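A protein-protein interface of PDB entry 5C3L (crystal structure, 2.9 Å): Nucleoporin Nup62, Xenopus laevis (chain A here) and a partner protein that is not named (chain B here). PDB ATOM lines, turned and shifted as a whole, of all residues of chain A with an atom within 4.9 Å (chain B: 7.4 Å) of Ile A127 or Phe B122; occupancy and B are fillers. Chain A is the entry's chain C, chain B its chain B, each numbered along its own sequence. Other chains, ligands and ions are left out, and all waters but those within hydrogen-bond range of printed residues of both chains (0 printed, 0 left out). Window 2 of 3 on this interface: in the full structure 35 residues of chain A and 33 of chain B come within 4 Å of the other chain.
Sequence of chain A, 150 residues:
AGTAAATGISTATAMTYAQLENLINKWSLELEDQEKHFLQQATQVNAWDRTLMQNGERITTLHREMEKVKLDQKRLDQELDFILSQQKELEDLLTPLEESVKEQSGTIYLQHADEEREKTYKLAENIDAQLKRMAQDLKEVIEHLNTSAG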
ATOM      1  N   LEU A 123       3.890 -11.132 -21.770  1.00  0.00           N
ATOM      2  CA  LEU A 123       4.041 -11.129 -20.331  1.00  0.00           C
ATOM      3  C   LEU A 123       2.848 -10.405 -19.699  1.00  0.00           C
ATOM      4  O   LEU A 123       2.341 -10.806 -18.651  1.00  0.00           O
ATOM      5  CB  LEU A 123       5.367 -10.469 -19.954  1.00  0.00           C
ATOM      6  CG  LEU A 123       5.671 -10.363 -18.467  1.00  0.00           C
ATOM      7  CD1 LEU A 123       5.485 -11.713 -17.745  1.00  0.00           C
ATOM      8  CD2 LEU A 123       7.080  -9.809 -18.295  1.00  0.00           C
ATOM      9  N   ALA A 124       2.385  -9.357 -20.379  1.00  0.00           N
ATOM     10  CA  ALA A 124       1.201  -8.608 -19.968  1.00  0.00           C
ATOM     11  C   ALA A 124      -0.063  -9.455 -20.129  1.00  0.00           C
ATOM     12  O   ALA A 124      -0.942  -9.435 -19.275  1.00  0.00           O
ATOM     13  CB  ALA A 124       1.093  -7.318 -20.787  1.00  0.00           C
ATOM     14  N   GLU A 125      -0.150 -10.193 -21.230  1.00  0.00           N
ATOM     15  CA  GLU A 125      -1.291 -11.065 -21.484  1.00  0.00           C
ATOM     16  C   GLU A 125      -1.437 -12.096 -20.372  1.00  0.00           C
ATOM     17  O   GLU A 125      -2.547 -12.384 -19.920  1.00  0.00           O
ATOM     18  CB  GLU A 125      -1.144 -11.774 -22.835  1.00  0.00           C
ATOM     19  CG  GLU A 125      -2.285 -12.732 -23.147  1.00  0.00           C
ATOM     20  CD  GLU A 125      -2.263 -13.247 -24.571  1.00  0.00           C
ATOM     21  OE1 GLU A 125      -1.386 -12.825 -25.350  1.00  0.00           O
ATOM     22  OE2 GLU A 125      -3.132 -14.074 -24.917  1.00  0.00           O
ATOM     23  N   ASN A 126      -0.308 -12.651 -19.937  1.00  0.00           N
ATOM     24  CA  ASN A 126      -0.307 -13.662 -18.885  1.00  0.00           C
ATOM     25  C   ASN A 126      -0.703 -13.086 -17.526  1.00  0.00           C
ATOM     26  O   ASN A 126      -1.525 -13.663 -16.816  1.00  0.00           O
ATOM     27  CB  ASN A 126       1.072 -14.318 -18.771  1.00  0.00           C
ATOM     28  CG  ASN A 126       1.394 -15.216 -19.948  1.00  0.00           C
ATOM     29  OD1 ASN A 126       0.497 -15.667 -20.664  1.00  0.00           O
ATOM     30  ND2 ASN A 126       2.676 -15.496 -20.146  1.00  0.00           N
ATOM     31  N   ILE A 127      -0.110 -11.947 -17.182  1.00  0.00           N
ATOM     32  CA  ILE A 127      -0.359 -11.289 -15.907  1.00  0.00           C
ATOM     33  C   ILE A 127      -1.842 -10.981 -15.773  1.00  0.00           C
ATOM     34  O   ILE A 127      -2.434 -11.151 -14.706  1.00  0.00           O
ATOM     35  CB  ILE A 127       0.474  -9.990 -15.780  1.00  0.00           C
ATOM     36  CG1 ILE A 127       1.953 -10.333 -15.624  1.00  0.00           C
ATOM     37  CG2 ILE A 127       0.033  -9.150 -14.579  1.00  0.00           C
ATOM     38  CD1 ILE A 127       2.902  -9.195 -15.965  1.00  0.00           C
ATOM     39  N   ASP A 128      -2.439 -10.545 -16.872  1.00  0.00           N
ATOM     40  CA  ASP A 128      -3.851 -10.207 -16.882  1.00  0.00           C
ATOM     41  C   ASP A 128      -4.669 -11.476 -16.702  1.00  0.00           C
ATOM     42  O   ASP A 128      -5.709 -11.475 -16.042  1.00  0.00           O
ATOM     43  CB  ASP A 128      -4.229  -9.499 -18.185  1.00  0.00           C
ATOM     44  CG  ASP A 128      -5.665  -8.999 -18.182  1.00  0.00           C
ATOM     45  OD1 ASP A 128      -6.101  -8.426 -17.158  1.00  0.00           O
ATOM     46  OD2 ASP A 128      -6.361  -9.201 -19.200  1.00  0.00           O
ATOM     47  N   ALA A 129      -4.184 -12.564 -17.287  1.00  0.00           N
ATOM     48  CA  ALA A 129      -4.834 -13.864 -17.156  1.00  0.00           C
ATOM     49  C   ALA A 129      -4.774 -14.372 -15.710  1.00  0.00           C
ATOM     50  O   ALA A 129      -5.739 -14.947 -15.205  1.00  0.00           O
ATOM     51  CB  ALA A 129      -4.198 -14.865 -18.095  1.00  0.00           C
ATOM     52  N   GLN A 130      -3.647 -14.132 -15.048  1.00  0.00           N
ATOM     53  CA  GLN A 130      -3.461 -14.524 -13.654  1.00  0.00           C
ATOM     54  C   GLN A 130      -4.352 -13.743 -12.696  1.00  0.00           C
ATOM     55  O   GLN A 130      -5.053 -14.336 -11.872  1.00  0.00           O
ATOM     56  CB  GLN A 130      -2.003 -14.330 -13.240  1.00  0.00           C
ATOM     57  CG  GLN A 130      -1.062 -15.367 -13.808  1.00  0.00           C
ATOM     58  CD  GLN A 130       0.316 -15.307 -13.186  1.00  0.00           C
ATOM     59  OE1 GLN A 130       0.490 -15.560 -11.987  1.00  0.00           O
ATOM     60  NE2 GLN A 130       1.308 -14.979 -14.001  1.00  0.00           N
ATOM     61  N   LEU A 131      -4.295 -12.416 -12.800  1.00  0.00           N
ATOM     62  CA  LEU A 131      -5.014 -11.518 -11.900  1.00  0.00           C
ATOM     63  C   LEU A 131      -6.520 -11.669 -12.033  1.00  0.00           C
ATOM     64  O   LEU A 131      -7.265 -11.392 -11.092  1.00  0.00           O
ATOM     65  CB  LEU A 131      -4.635 -10.068 -12.175  1.00  0.00           C
ATOM     66  CG  LEU A 131      -3.229  -9.600 -11.817  1.00  0.00           C
ATOM     67  CD1 LEU A 131      -3.026  -8.160 -12.256  1.00  0.00           C
ATOM     68  CD2 LEU A 131      -2.990  -9.747 -10.328  1.00  0.00           C
ATOM     69  N   LYS A 132      -6.968 -12.082 -13.210  1.00  0.00           N
ATOM     70  CA  LYS A 132      -8.380 -12.328 -13.428  1.00  0.00           C
ATOM     71  C   LYS A 132      -8.803 -13.646 -12.791  1.00  0.00           C
ATOM     72  O   LYS A 132      -9.919 -13.766 -12.283  1.00  0.00           O
ATOM     73  CB  LYS A 132      -8.694 -12.323 -14.922  1.00  0.00           C
ATOM     74  CG  LYS A 132      -9.029 -10.948 -15.417  1.00  0.00           C
ATOM     75  CD  LYS A 132      -9.023 -10.834 -16.917  1.00  0.00           C
ATOM     76  CE  LYS A 132      -9.219  -9.384 -17.325  1.00  0.00           C
ATOM     77  NZ  LYS A 132      -8.935  -9.186 -18.754  1.00  0.00           N
ATOM     78  N   PHE B 115      -1.729   0.816 -22.416  1.00  0.00           N
ATOM     79  CA  PHE B 115      -0.803  -0.084 -21.736  1.00  0.00           C
ATOM     80  C   PHE B 115      -0.245   0.569 -20.478  1.00  0.00           C
ATOM     81  O   PHE B 115      -0.149  -0.077 -19.441  1.00  0.00           O
ATOM     82  CB  PHE B 115       0.327  -0.528 -22.688  1.00  0.00           C
ATOM     83  CG  PHE B 115      -0.136  -1.484 -23.765  1.00  0.00           C
ATOM     84  CD1 PHE B 115      -0.516  -2.776 -23.452  1.00  0.00           C
ATOM     85  CD2 PHE B 115      -0.219  -1.081 -25.086  1.00  0.00           C
ATOM     86  CE1 PHE B 115      -0.956  -3.645 -24.438  1.00  0.00           C
ATOM     87  CE2 PHE B 115      -0.659  -1.956 -26.073  1.00  0.00           C
ATOM     88  CZ  PHE B 115      -1.026  -3.227 -25.749  1.00  0.00           C
ATOM     89  N   HIS B 116       0.096   1.849 -20.549  1.00  0.00           N
ATOM     90  CA  HIS B 116       0.591   2.551 -19.369  1.00  0.00           C
ATOM     91  C   HIS B 116      -0.472   2.495 -18.256  1.00  0.00           C
ATOM     92  O   HIS B 116      -0.161   2.210 -17.101  1.00  0.00           O
ATOM     93  CB  HIS B 116       0.948   3.991 -19.718  1.00  0.00           C
ATOM     94  CG  HIS B 116       1.252   4.845 -18.527  1.00  0.00           C
ATOM     95  ND1 HIS B 116       2.530   5.025 -18.041  1.00  0.00           N
ATOM     96  CD2 HIS B 116       0.437   5.575 -17.726  1.00  0.00           C
ATOM     97  CE1 HIS B 116       2.490   5.828 -16.993  1.00  0.00           C
ATOM     98  NE2 HIS B 116       1.231   6.175 -16.779  1.00  0.00           N
ATOM     99  N   THR B 117      -1.725   2.749 -18.626  1.00  0.00           N
ATOM    100  CA  THR B 117      -2.858   2.625 -17.715  1.00  0.00           C
ATOM    101  C   THR B 117      -3.005   1.178 -17.238  1.00  0.00           C
ATOM    102  O   THR B 117      -3.395   0.927 -16.099  1.00  0.00           O
ATOM    103  CB  THR B 117      -4.181   3.081 -18.399  1.00  0.00           C
ATOM    104  OG1 THR B 117      -4.060   4.443 -18.810  1.00  0.00           O
ATOM    105  CG2 THR B 117      -5.400   2.950 -17.468  1.00  0.00           C
ATOM    106  N   LEU B 118      -2.688   0.234 -18.119  1.00  0.00           N
ATOM    107  CA  LEU B 118      -2.911  -1.189 -17.863  1.00  0.00           C
ATOM    108  C   LEU B 118      -2.037  -1.714 -16.723  1.00  0.00           C
ATOM    109  O   LEU B 118      -2.509  -2.472 -15.874  1.00  0.00           O
ATOM    110  CB  LEU B 118      -2.648  -2.000 -19.141  1.00  0.00           C
ATOM    111  CG  LEU B 118      -2.772  -3.526 -19.091  1.00  0.00           C
ATOM    112  CD1 LEU B 118      -4.194  -3.990 -19.326  1.00  0.00           C
ATOM    113  CD2 LEU B 118      -1.811  -4.171 -20.095  1.00  0.00           C
ATOM    114  N   VAL B 119      -0.765  -1.315 -16.705  1.00  0.00           N
ATOM    115  CA  VAL B 119       0.177  -1.814 -15.700  1.00  0.00           C
ATOM    116  C   VAL B 119      -0.018  -1.172 -14.334  1.00  0.00           C
ATOM    117  O   VAL B 119       0.262  -1.798 -13.316  1.00  0.00           O
ATOM    118  CB  VAL B 119       1.648  -1.591 -16.110  1.00  0.00           C
ATOM    119  CG1 VAL B 119       1.935  -2.281 -17.421  1.00  0.00           C
ATOM    120  CG2 VAL B 119       1.976  -0.097 -16.176  1.00  0.00           C
ATOM    121  N   GLN B 120      -0.466   0.078 -14.305  1.00  0.00           N
ATOM    122  CA  GLN B 120      -0.735   0.715 -13.029  1.00  0.00           C
ATOM    123  C   GLN B 120      -2.045   0.150 -12.499  1.00  0.00           C
ATOM    124  O   GLN B 120      -2.288   0.150 -11.299  1.00  0.00           O
ATOM    125  CB  GLN B 120      -0.772   2.244 -13.155  1.00  0.00           C
ATOM    126  CG  GLN B 120      -1.905   2.820 -13.985  1.00  0.00           C
ATOM    127  CD  GLN B 120      -1.844   4.343 -14.083  1.00  0.00           C
ATOM    128  OE1 GLN B 120      -0.757   4.928 -14.132  1.00  0.00           O
ATOM    129  NE2 GLN B 120      -3.015   4.990 -14.115  1.00  0.00           N
ATOM    130  N   GLN B 121      -2.871  -0.373 -13.395  1.00  0.00           N
ATOM    131  CA  GLN B 121      -4.085  -1.062 -12.988  1.00  0.00           C
ATOM    132  C   GLN B 121      -3.720  -2.431 -12.412  1.00  0.00           C
ATOM    133  O   GLN B 121      -4.369  -2.916 -11.494  1.00  0.00           O
ATOM    134  CB  GLN B 121      -5.039  -1.202 -14.172  1.00  0.00           C
ATOM    135  CG  GLN B 121      -6.383  -1.829 -13.848  1.00  0.00           C
ATOM    136  CD  GLN B 121      -7.179  -2.162 -15.102  1.00  0.00           C
ATOM    137  OE1 GLN B 121      -7.609  -1.272 -15.836  1.00  0.00           O
ATOM    138  NE2 GLN B 121      -7.363  -3.450 -15.360  1.00  0.00           N
ATOM    139  N   PHE B 122      -2.678  -3.051 -12.962  1.00  0.00           N
ATOM    140  CA  PHE B 122      -2.154  -4.310 -12.432  1.00  0.00           C
ATOM    141  C   PHE B 122      -1.613  -4.120 -11.020  1.00  0.00           C
ATOM    142  O   PHE B 122      -1.937  -4.881 -10.112  1.00  0.00           O
ATOM    143  CB  PHE B 122      -1.032  -4.857 -13.324  1.00  0.00           C
ATOM    144  CG  PHE B 122      -1.495  -5.437 -14.641  1.00  0.00           C
ATOM    145  CD1 PHE B 122      -2.788  -5.897 -14.812  1.00  0.00           C
ATOM    146  CD2 PHE B 122      -0.611  -5.553 -15.704  1.00  0.00           C
ATOM    147  CE1 PHE B 122      -3.194  -6.445 -16.017  1.00  0.00           C
ATOM    148  CE2 PHE B 122      -1.015  -6.099 -16.908  1.00  0.00           C
ATOM    149  CZ  PHE B 122      -2.309  -6.546 -17.062  1.00  0.00           C
ATOM    150  N   GLU B 123      -0.768  -3.106 -10.860  1.00  0.00           N
ATOM    151  CA  GLU B 123      -0.176  -2.750  -9.573  1.00  0.00           C
ATOM    152  C   GLU B 123      -1.239  -2.442  -8.519  1.00  0.00           C
ATOM    153  O   GLU B 123      -1.102  -2.794  -7.348  1.00  0.00           O
ATOM    154  CB  GLU B 123       0.742  -1.545  -9.748  1.00  0.00           C
ATOM    155  CG  GLU B 123       2.209  -1.899  -9.775  1.00  0.00           C
ATOM    156  CD  GLU B 123       3.057  -0.842 -10.454  1.00  0.00           C
ATOM    157  OE1 GLU B 123       2.539   0.269 -10.713  1.00  0.00           O
ATOM    158  OE2 GLU B 123       4.244  -1.130 -10.736  1.00  0.00           O
ATOM    159  N   VAL B 124      -2.297  -1.771  -8.954  1.00  0.00           N
ATOM    160  CA  VAL B 124      -3.434  -1.464  -8.102  1.00  0.00           C
ATOM    161  C   VAL B 124      -4.277  -2.713  -7.816  1.00  0.00           C
ATOM    162  O   VAL B 124      -5.011  -2.768  -6.838  1.00  0.00           O
ATOM    163  CB  VAL B 124      -4.320  -0.381  -8.756  1.00  0.00           C
ATOM    164  CG1 VAL B 124      -5.700  -0.339  -8.119  1.00  0.00           C
ATOM    165  CG2 VAL B 124      -3.656   0.968  -8.650  1.00  0.00           C
ATOM    166  N   GLN B 125      -4.171  -3.720  -8.670  1.00  0.00           N
ATOM    167  CA  GLN B 125      -5.024  -4.897  -8.549  1.00  0.00           C
ATOM    168  C   GLN B 125      -4.527  -5.901  -7.527  1.00  0.00           C
ATOM    169  O   GLN B 125      -5.315  -6.391  -6.722  1.00  0.00           O
ATOM    170  CB  GLN B 125      -5.169  -5.585  -9.901  1.00  0.00           C
ATOM    171  CG  GLN B 125      -6.549  -5.425 -10.507  1.00  0.00           C
ATOM    172  CD  GLN B 125      -6.568  -5.665 -11.998  1.00  0.00           C
ATOM    173  OE1 GLN B 125      -5.643  -5.280 -12.713  1.00  0.00           O
ATOM    174  NE2 GLN B 125      -7.623  -6.309 -12.477  1.00  0.00           N
ATOM    175  N   LEU B 126      -3.241  -6.230  -7.547  1.00  0.00           N
ATOM    176  CA  LEU B 126      -2.752  -7.221  -6.591  1.00  0.00           C
ATOM    177  C   LEU B 126      -2.645  -6.590  -5.206  1.00  0.00           C
ATOM    178  O   LEU B 126      -2.615  -7.298  -4.200  1.00  0.00           O
ATOM    179  CB  LEU B 126      -1.406  -7.827  -7.023  1.00  0.00           C
ATOM    180  CG  LEU B 126      -0.341  -6.934  -7.652  1.00  0.00           C
ATOM    181  CD1 LEU B 126      -0.236  -5.596  -6.929  1.00  0.00           C
ATOM    182  CD2 LEU B 126       0.991  -7.670  -7.649  1.00  0.00           C
ATOM    183  N   GLN B 127      -2.612  -5.260  -5.148  1.00  0.00           N
ATOM    184  CA  GLN B 127      -2.608  -4.568  -3.866  1.00  0.00           C
ATOM    185  C   GLN B 127      -3.983  -4.741  -3.217  1.00  0.00           C
ATOM    186  O   GLN B 127      -4.091  -4.999  -2.020  1.00  0.00           O
ATOM    187  CB  GLN B 127      -2.258  -3.089  -4.047  1.00  0.00           C
ATOM    188  CG  GLN B 127      -1.246  -2.562  -3.034  1.00  0.00           C
ATOM    189  CD  GLN B 127      -0.662  -1.209  -3.424  1.00  0.00           C
ATOM    190  OE1 GLN B 127       0.521  -0.943  -3.194  1.00  0.00           O
ATOM    191  NE2 GLN B 127      -1.490  -0.346  -4.007  1.00  0.00           N
ATOM    192  N   GLN B 128      -5.027  -4.610  -4.030  1.00  0.00           N
ATOM    193  CA  GLN B 128      -6.388  -4.900  -3.598  1.00  0.00           C
ATOM    194  C   GLN B 128      -6.533  -6.354  -3.190  1.00  0.00           C
ATOM    195  O   GLN B 128      -7.085  -6.662  -2.140  1.00  0.00           O
ATOM    196  CB  GLN B 128      -7.385  -4.594  -4.714  1.00  0.00           C
ATOM    197  CG  GLN B 128      -7.528  -3.137  -5.066  1.00  0.00           C
ATOM    198  CD  GLN B 128      -8.435  -2.933  -6.256  1.00  0.00           C
ATOM    199  OE1 GLN B 128      -9.089  -3.870  -6.722  1.00  0.00           O
ATOM    200  NE2 GLN B 128      -8.497  -1.700  -6.746  1.00  0.00           N
ATOM    201  N   TYR B 129      -6.038  -7.243  -4.046  1.00  0.00           N
ATOM    202  CA  TYR B 129      -6.157  -8.686  -3.840  1.00  0.00           C
ATOM    203  C   TYR B 129      -5.416  -9.149  -2.576  1.00  0.00           C
ATOM    204  O   TYR B 129      -5.935  -9.965  -1.819  1.00  0.00           O
ATOM    205  CB  TYR B 129      -5.646  -9.428  -5.082  1.00  0.00           C
ATOM    206  CG  TYR B 129      -6.480  -9.165  -6.328  1.00  0.00           C
ATOM    207  CD1 TYR B 129      -7.859  -9.034  -6.250  1.00  0.00           C
ATOM    208  CD2 TYR B 129      -5.887  -9.050  -7.579  1.00  0.00           C
ATOM    209  CE1 TYR B 129      -8.624  -8.790  -7.380  1.00  0.00           C
ATOM    210  CE2 TYR B 129      -6.647  -8.804  -8.717  1.00  0.00           C
ATOM    211  CZ  TYR B 129      -8.015  -8.675  -8.609  1.00  0.00           C
ATOM    212  OH  TYR B 129      -8.775  -8.430  -9.734  1.00  0.00           O
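The backbone carbonyl oxygen (O) of Gln B121 lies close to the side-chain amide oxygen (OE1) of Gln B125 (2.9 Å). The side-chain carboxylate of Asp A128 lies within salt-bridge range of the side-chain amino group of Lys A132 (2.6 Å).
Ala A124 touches Phe B122. Ile A127 touches Phe B122 (CG2 to CD2, 3.8 Å). CB of Asp A128 touches CZ of Phe B122, at 3.7 Å. Phe B122 touches Leu A131. Leu A131 touches Gln B125 (CD1 to OE1, 3.9 Å). O of Leu A131 touches CE2 of Tyr B129 (3.6 Å).
Of the 15 printed residues of chain B, 3 touch a printed residue of chain A. Hydrophobic or aromatic side chains of chain B that line the printed part of chain A: Phe B122 and Tyr B129. Of the 10 printed residues of chain A, 4 touch a printed residue of chain B. Among the printed residues, 6 pairs touch across the chains. Among the printed residues, no Asp or Glu carboxylate lies within 4 Å of a Lys or Arg side-chain nitrogen of the other chain.
Ile A127 touches one residue of chain B. Of chain A, only Ala A124 (3.9 Å), Ile A127 (3.8 Å), Asp A128 (3.7 Å) and Leu A131 (3.4 Å) come within 4 Å of Phe B122. Of the printed residues of chain B, Asp A128 touches Phe B122 (3.7 Å). Of the printed residues of chain A, Tyr B129 touches Leu A131. Of the printed residues of chain A, Gln B125 touches Leu A131 (3.9 Å). Glu B123 touches none of the printed residues of chain A. Gln B128 touches none of the printed residues of chain A. The nearest residue of chain B that does not touch Ile A127 is Gln B125 (7.0 Å). The nearest printed residue of chain A that does not touch Phe B122 is Glu A125 (5.9 Å).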
